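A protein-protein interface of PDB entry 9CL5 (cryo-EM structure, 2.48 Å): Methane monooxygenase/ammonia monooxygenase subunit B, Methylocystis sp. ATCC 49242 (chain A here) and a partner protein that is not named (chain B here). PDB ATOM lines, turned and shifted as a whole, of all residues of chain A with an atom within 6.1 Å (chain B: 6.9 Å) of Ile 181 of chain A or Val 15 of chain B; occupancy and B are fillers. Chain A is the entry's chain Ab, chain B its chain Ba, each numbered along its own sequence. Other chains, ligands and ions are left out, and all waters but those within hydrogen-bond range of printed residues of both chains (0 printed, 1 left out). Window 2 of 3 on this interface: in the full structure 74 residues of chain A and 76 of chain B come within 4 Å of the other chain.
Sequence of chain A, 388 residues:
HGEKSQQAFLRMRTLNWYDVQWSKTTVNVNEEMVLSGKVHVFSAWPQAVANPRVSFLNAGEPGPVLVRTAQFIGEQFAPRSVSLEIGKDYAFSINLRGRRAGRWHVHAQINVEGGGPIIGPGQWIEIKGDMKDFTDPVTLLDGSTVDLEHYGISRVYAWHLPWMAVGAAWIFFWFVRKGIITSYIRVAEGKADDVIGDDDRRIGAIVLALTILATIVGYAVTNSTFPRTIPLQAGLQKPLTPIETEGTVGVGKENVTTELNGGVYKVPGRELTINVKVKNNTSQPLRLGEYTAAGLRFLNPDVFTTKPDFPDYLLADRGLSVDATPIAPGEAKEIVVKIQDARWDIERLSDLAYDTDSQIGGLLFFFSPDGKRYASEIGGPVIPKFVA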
ATOM      1  N   GLY A 179       6.352   3.151  16.560  1.00  0.00           N
ATOM      2  CA  GLY A 179       7.740   3.523  16.735  1.00  0.00           C
ATOM      3  C   GLY A 179       8.433   3.761  15.408  1.00  0.00           C
ATOM      4  O   GLY A 179       7.881   3.552  14.328  1.00  0.00           O
ATOM      5  N   ILE A 180       9.681   4.208  15.499  1.00  0.00           N
ATOM      6  CA  ILE A 180      10.483   4.559  14.336  1.00  0.00           C
ATOM      7  C   ILE A 180      11.561   3.514  14.068  1.00  0.00           C
ATOM      8  O   ILE A 180      11.681   3.010  12.952  1.00  0.00           O
ATOM      9  CB  ILE A 180      11.101   5.965  14.497  1.00  0.00           C
ATOM     10  CG1 ILE A 180      10.005   7.031  14.510  1.00  0.00           C
ATOM     11  CG2 ILE A 180      12.104   6.241  13.393  1.00  0.00           C
ATOM     12  CD1 ILE A 180      10.522   8.432  14.712  1.00  0.00           C
ATOM     13  N   ILE A 181      12.361   3.184  15.082  1.00  0.00           N
ATOM     14  CA  ILE A 181      13.409   2.181  14.905  1.00  0.00           C
ATOM     15  C   ILE A 181      12.800   0.804  14.676  1.00  0.00           C
ATOM     16  O   ILE A 181      13.228   0.063  13.781  1.00  0.00           O
ATOM     17  CB  ILE A 181      14.363   2.189  16.114  1.00  0.00           C
ATOM     18  CG1 ILE A 181      15.256   3.431  16.082  1.00  0.00           C
ATOM     19  CG2 ILE A 181      15.205   0.923  16.145  1.00  0.00           C
ATOM     20  CD1 ILE A 181      16.118   3.598  17.311  1.00  0.00           C
ATOM     21  N   THR A 182      11.795   0.437  15.475  1.00  0.00           N
ATOM     22  CA  THR A 182      11.162  -0.870  15.320  1.00  0.00           C
ATOM     23  C   THR A 182      10.483  -0.998  13.961  1.00  0.00           C
ATOM     24  O   THR A 182      10.607  -2.029  13.291  1.00  0.00           O
ATOM     25  CB  THR A 182      10.152  -1.102  16.444  1.00  0.00           C
ATOM     26  OG1 THR A 182      10.786  -0.876  17.710  1.00  0.00           O
ATOM     27  CG2 THR A 182       9.626  -2.524  16.399  1.00  0.00           C
ATOM     28  N   SER A 183       9.764   0.044  13.539  1.00  0.00           N
ATOM     29  CA  SER A 183       9.118   0.019  12.232  1.00  0.00           C
ATOM     30  C   SER A 183      10.146  -0.046  11.113  1.00  0.00           C
ATOM     31  O   SER A 183       9.956  -0.765  10.124  1.00  0.00           O
ATOM     32  CB  SER A 183       8.221   1.242  12.067  1.00  0.00           C
ATOM     33  OG  SER A 183       6.971   1.043  12.702  1.00  0.00           O
ATOM     34  N   TYR A 184      11.245   0.700  11.249  1.00  0.00           N
ATOM     35  CA  TYR A 184      12.302   0.644  10.247  1.00  0.00           C
ATOM     36  C   TYR A 184      12.882  -0.758  10.133  1.00  0.00           C
ATOM     37  O   TYR A 184      13.099  -1.258   9.024  1.00  0.00           O
ATOM     38  CB  TYR A 184      13.410   1.644  10.584  1.00  0.00           C
ATOM     39  CG  TYR A 184      14.615   1.490   9.691  1.00  0.00           C
ATOM     40  CD1 TYR A 184      14.660   2.104   8.449  1.00  0.00           C
ATOM     41  CD2 TYR A 184      15.698   0.708  10.076  1.00  0.00           C
ATOM     42  CE1 TYR A 184      15.749   1.954   7.623  1.00  0.00           C
ATOM     43  CE2 TYR A 184      16.785   0.549   9.255  1.00  0.00           C
ATOM     44  CZ  TYR A 184      16.808   1.177   8.032  1.00  0.00           C
ATOM     45  OH  TYR A 184      17.891   1.024   7.211  1.00  0.00           O
ATOM     46  N   ILE A 185      13.153  -1.404  11.268  1.00  0.00           N
ATOM     47  CA  ILE A 185      13.737  -2.740  11.233  1.00  0.00           C
ATOM     48  C   ILE A 185      12.746  -3.740  10.653  1.00  0.00           C
ATOM     49  O   ILE A 185      13.126  -4.636   9.891  1.00  0.00           O
ATOM     50  CB  ILE A 185      14.215  -3.151  12.637  1.00  0.00           C
ATOM     51  CG1 ILE A 185      15.398  -2.282  13.068  1.00  0.00           C
ATOM     52  CG2 ILE A 185      14.618  -4.614  12.659  1.00  0.00           C
ATOM     53  CD1 ILE A 185      15.886  -2.563  14.468  1.00  0.00           C
ATOM     54  N   ARG A 186      11.462  -3.602  10.995  1.00  0.00           N
ATOM     55  CA  ARG A 186      10.454  -4.499  10.440  1.00  0.00           C
ATOM     56  C   ARG A 186      10.354  -4.354   8.927  1.00  0.00           C
ATOM     57  O   ARG A 186      10.290  -5.354   8.204  1.00  0.00           O
ATOM     58  CB  ARG A 186       9.099  -4.236  11.094  1.00  0.00           C
ATOM     59  CG  ARG A 186       8.834  -5.092  12.316  1.00  0.00           C
ATOM     60  CD  ARG A 186       7.363  -5.119  12.677  1.00  0.00           C
ATOM     61  NE  ARG A 186       7.138  -5.754  13.970  1.00  0.00           N
ATOM     62  CZ  ARG A 186       6.871  -5.100  15.090  1.00  0.00           C
ATOM     63  NH1 ARG A 186       6.778  -3.780  15.114  1.00  0.00           N
ATOM     64  NH2 ARG A 186       6.694  -5.784  16.215  1.00  0.00           N
ATOM     65  N   PHE B   5      24.144  -3.654  23.603  1.00  0.00           N
ATOM     66  CA  PHE B   5      23.449  -3.422  24.860  1.00  0.00           C
ATOM     67  C   PHE B   5      23.685  -4.593  25.804  1.00  0.00           C
ATOM     68  O   PHE B   5      23.670  -5.753  25.384  1.00  0.00           O
ATOM     69  CB  PHE B   5      21.950  -3.238  24.625  1.00  0.00           C
ATOM     70  CG  PHE B   5      21.622  -2.235  23.559  1.00  0.00           C
ATOM     71  CD1 PHE B   5      21.777  -0.883  23.791  1.00  0.00           C
ATOM     72  CD2 PHE B   5      21.164  -2.650  22.320  1.00  0.00           C
ATOM     73  CE1 PHE B   5      21.480   0.038  22.810  1.00  0.00           C
ATOM     74  CE2 PHE B   5      20.865  -1.732  21.336  1.00  0.00           C
ATOM     75  CZ  PHE B   5      21.023  -0.385  21.581  1.00  0.00           C
ATOM     76  N   ALA B   9      16.467  -4.370  29.070  1.00  0.00           N
ATOM     77  CA  ALA B   9      15.930  -3.068  29.448  1.00  0.00           C
ATOM     78  C   ALA B   9      16.771  -1.935  28.880  1.00  0.00           C
ATOM     79  O   ALA B   9      16.234  -0.907  28.453  1.00  0.00           O
ATOM     80  CB  ALA B   9      15.840  -2.961  30.970  1.00  0.00           C
ATOM     81  N   GLU B  10      18.097  -2.095  28.881  1.00  0.00           N
ATOM     82  CA  GLU B  10      18.961  -1.071  28.306  1.00  0.00           C
ATOM     83  C   GLU B  10      18.687  -0.892  26.821  1.00  0.00           C
ATOM     84  O   GLU B  10      18.610   0.240  26.327  1.00  0.00           O
ATOM     85  CB  GLU B  10      20.428  -1.429  28.539  1.00  0.00           C
ATOM     86  CG  GLU B  10      21.394  -0.364  28.061  1.00  0.00           C
ATOM     87  CD  GLU B  10      22.842  -0.757  28.256  1.00  0.00           C
ATOM     88  OE1 GLU B  10      23.097  -1.871  28.759  1.00  0.00           O
ATOM     89  OE2 GLU B  10      23.726   0.052  27.907  1.00  0.00           O
ATOM     90  N   ALA B  11      18.526  -2.000  26.093  1.00  0.00           N
ATOM     91  CA  ALA B  11      18.216  -1.917  24.670  1.00  0.00           C
ATOM     92  C   ALA B  11      16.890  -1.207  24.439  1.00  0.00           C
ATOM     93  O   ALA B  11      16.789  -0.318  23.585  1.00  0.00           O
ATOM     94  CB  ALA B  11      18.189  -3.319  24.061  1.00  0.00           C
ATOM     95  N   ALA B  12      15.861  -1.579  25.207  1.00  0.00           N
ATOM     96  CA  ALA B  12      14.551  -0.958  25.033  1.00  0.00           C
ATOM     97  C   ALA B  12      14.597   0.535  25.335  1.00  0.00           C
ATOM     98  O   ALA B  12      14.041   1.347  24.583  1.00  0.00           O
ATOM     99  CB  ALA B  12      13.521  -1.654  25.922  1.00  0.00           C
ATOM    100  N   GLY B  13      15.269   0.918  26.423  1.00  0.00           N
ATOM    101  CA  GLY B  13      15.352   2.324  26.774  1.00  0.00           C
ATOM    102  C   GLY B  13      16.127   3.137  25.757  1.00  0.00           C
ATOM    103  O   GLY B  13      15.721   4.246  25.396  1.00  0.00           O
ATOM    104  N   CYS B  14      17.255   2.602  25.281  1.00  0.00           N
ATOM    105  CA  CYS B  14      18.027   3.305  24.265  1.00  0.00           C
ATOM    106  C   CYS B  14      17.227   3.464  22.981  1.00  0.00           C
ATOM    107  O   CYS B  14      17.258   4.527  22.350  1.00  0.00           O
ATOM    108  CB  CYS B  14      19.338   2.570  23.993  1.00  0.00           C
ATOM    109  SG  CYS B  14      20.302   3.257  22.626  1.00  0.00           S
ATOM    110  N   VAL B  15      16.501   2.417  22.578  1.00  0.00           N
ATOM    111  CA  VAL B  15      15.695   2.501  21.364  1.00  0.00           C
ATOM    112  C   VAL B  15      14.611   3.560  21.517  1.00  0.00           C
ATOM    113  O   VAL B  15      14.383   4.365  20.608  1.00  0.00           O
ATOM    114  CB  VAL B  15      15.104   1.122  21.018  1.00  0.00           C
ATOM    115  CG1 VAL B  15      14.001   1.258  19.981  1.00  0.00           C
ATOM    116  CG2 VAL B  15      16.194   0.200  20.506  1.00  0.00           C
ATOM    117  N   GLN B  16      13.939   3.592  22.672  1.00  0.00           N
ATOM    118  CA  GLN B  16      12.899   4.594  22.891  1.00  0.00           C
ATOM    119  C   GLN B  16      13.472   6.010  22.869  1.00  0.00           C
ATOM    120  O   GLN B  16      12.897   6.915  22.245  1.00  0.00           O
ATOM    121  CB  GLN B  16      12.185   4.316  24.213  1.00  0.00           C
ATOM    122  CG  GLN B  16      11.230   5.408  24.656  1.00  0.00           C
ATOM    123  CD  GLN B  16      10.940   5.354  26.143  1.00  0.00           C
ATOM    124  OE1 GLN B  16      11.267   4.376  26.814  1.00  0.00           O
ATOM    125  NE2 GLN B  16      10.321   6.407  26.664  1.00  0.00           N
ATOM    126  N   THR B  17      14.610   6.216  23.537  1.00  0.00           N
ATOM    127  CA  THR B  17      15.215   7.544  23.576  1.00  0.00           C
ATOM    128  C   THR B  17      15.621   8.004  22.181  1.00  0.00           C
ATOM    129  O   THR B  17      15.314   9.133  21.775  1.00  0.00           O
ATOM    130  CB  THR B  17      16.425   7.538  24.513  1.00  0.00           C
ATOM    131  OG1 THR B  17      16.074   6.887  25.739  1.00  0.00           O
ATOM    132  CG2 THR B  17      16.872   8.958  24.814  1.00  0.00           C
ATOM    133  N   VAL B  18      16.296   7.134  21.427  1.00  0.00           N
ATOM    134  CA  VAL B  18      16.719   7.489  20.077  1.00  0.00           C
ATOM    135  C   VAL B  18      15.513   7.719  19.181  1.00  0.00           C
ATOM    136  O   VAL B  18      15.548   8.578  18.295  1.00  0.00           O
ATOM    137  CB  VAL B  18      17.665   6.411  19.511  1.00  0.00           C
ATOM    138  CG1 VAL B  18      18.044   6.728  18.075  1.00  0.00           C
ATOM    139  CG2 VAL B  18      18.912   6.313  20.368  1.00  0.00           C
ATOM    140  N   ASP B  19      14.425   6.975  19.399  1.00  0.00           N
ATOM    141  CA  ASP B  19      13.190   7.230  18.666  1.00  0.00           C
ATOM    142  C   ASP B  19      12.699   8.649  18.911  1.00  0.00           C
ATOM    143  O   ASP B  19      12.337   9.369  17.971  1.00  0.00           O
ATOM    144  CB  ASP B  19      12.120   6.221  19.088  1.00  0.00           C
ATOM    145  CG  ASP B  19      12.017   5.049  18.141  1.00  0.00           C
ATOM    146  OD1 ASP B  19      12.606   5.124  17.046  1.00  0.00           O
ATOM    147  OD2 ASP B  19      11.345   4.058  18.491  1.00  0.00           O
ATOM    148  N   TRP B  20      12.689   9.069  20.180  1.00  0.00           N
ATOM    149  CA  TRP B  20      12.245  10.421  20.509  1.00  0.00           C
ATOM    150  C   TRP B  20      13.118  11.474  19.833  1.00  0.00           C
ATOM    151  O   TRP B  20      12.607  12.420  19.215  1.00  0.00           O
ATOM    152  CB  TRP B  20      12.248  10.621  22.025  1.00  0.00           C
ATOM    153  CG  TRP B  20      10.990  10.182  22.699  1.00  0.00           C
ATOM    154  CD1 TRP B  20      10.842   9.127  23.548  1.00  0.00           C
ATOM    155  CD2 TRP B  20       9.699  10.789  22.583  1.00  0.00           C
ATOM    156  NE1 TRP B  20       9.538   9.038  23.968  1.00  0.00           N
ATOM    157  CE2 TRP B  20       8.816  10.048  23.389  1.00  0.00           C
ATOM    158  CE3 TRP B  20       9.204  11.888  21.875  1.00  0.00           C
ATOM    159  CZ2 TRP B  20       7.467  10.368  23.509  1.00  0.00           C
ATOM    160  CZ3 TRP B  20       7.866  12.205  21.994  1.00  0.00           C
ATOM    161  CH2 TRP B  20       7.013  11.448  22.804  1.00  0.00           C
ATOM    162  N   LEU B  22      15.118  11.191  17.188  1.00  0.00           N
ATOM    163  CA  LEU B  22      14.962  11.160  15.739  1.00  0.00           C
ATOM    164  C   LEU B  22      13.670  11.840  15.313  1.00  0.00           C
ATOM    165  O   LEU B  22      13.658  12.621  14.353  1.00  0.00           O
ATOM    166  CB  LEU B  22      14.991   9.720  15.232  1.00  0.00           C
ATOM    167  CG  LEU B  22      16.340   9.004  15.194  1.00  0.00           C
ATOM    168  CD1 LEU B  22      16.139   7.517  14.970  1.00  0.00           C
ATOM    169  CD2 LEU B  22      17.227   9.599  14.120  1.00  0.00           C
ATOM    170  N   PHE B  80       9.135   3.329   6.832  1.00  0.00           N
ATOM    171  CA  PHE B  80       8.623   2.923   8.134  1.00  0.00           C
ATOM    172  C   PHE B  80       7.185   2.428   8.121  1.00  0.00           C
ATOM    173  O   PHE B  80       6.744   1.886   9.138  1.00  0.00           O
ATOM    174  CB  PHE B  80       8.716   4.087   9.134  1.00  0.00           C
ATOM    175  CG  PHE B  80      10.068   4.739   9.195  1.00  0.00           C
ATOM    176  CD1 PHE B  80      10.390   5.776   8.334  1.00  0.00           C
ATOM    177  CD2 PHE B  80      11.010   4.329  10.120  1.00  0.00           C
ATOM    178  CE1 PHE B  80      11.625   6.378   8.387  1.00  0.00           C
ATOM    179  CE2 PHE B  80      12.247   4.931  10.179  1.00  0.00           C
ATOM    180  CZ  PHE B  80      12.556   5.956   9.311  1.00  0.00           C
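Ile 181 of chain A touches just these residues of chain B: Val 15 (3.8 Å), Val 18 (3.8 Å) and Asp 19 (2.8 Å). Of chain A, only Ile 181 (3.8 Å) comes within 4 Å of Val 15 of chain B. Of the printed residues of chain B, Ile 180 of chain A touches Asp 19 and Phe 80. Of the printed residues of chain A, Val 18 of chain B touches Ile 181 (3.8 Å). Printed residues of chain A within 4 Å of Asp 19 of chain B: Ile 180 (3.1 Å) and Ile 181 (2.8 Å). Of the printed residues of chain A, Phe 80 of chain B touches Ile 180, Ser 183 and Tyr 184. Gly 179 of chain A touches none of the printed residues of chain B. The nearest residue of chain B that does not touch Ile 181 of chain A is Leu 22 of chain B (4.3 Å).
The side-chain hydroxyl (OG) of Ser 183 of chain A sits at hydrogen-bond distance from the backbone carbonyl oxygen (O) of Gly 179 of chain A (3.1 Å).
Hydrophobic or aromatic side chains of chain A within 4 Å of the printed part of chain B: Ile 180, Ile 181 and Tyr 184. Hydrophobic or aromatic side chains of chain B within 4 Å of the printed part of chain A: Val 15, Val 18 and Phe 80. Among the printed residues, 7 pairs touch across the chains. Among the printed residues, no Asp or Glu carboxylate lies within 4 Å of a Lys or Arg side-chain nitrogen of the other chain.
Among the printed residues, merely in contact across the chains: Ile 180 of chain A with Phe 80 of chain B (3.2 Å), Ile 181 of chain A with Val 15 of chain B (3.8 Å), Ile 181 of chain A with Val 18 of chain B (3.8 Å), Ser 183 of chain A with Phe 80 of chain B (3.3 Å) and Tyr 184 of chain A with Phe 80 of chain B (3.5 Å).
The side-chain carboxylate (OD2) of Asp 19 of chain B is in hydrogen-bond range of the backbone NH (N) of Ile 180 of chain A (3.4 Å). OD1 of Asp 19 of chain B sits at hydrogen-bond distance from N of Ile 181 of chain A (2.8 Å).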
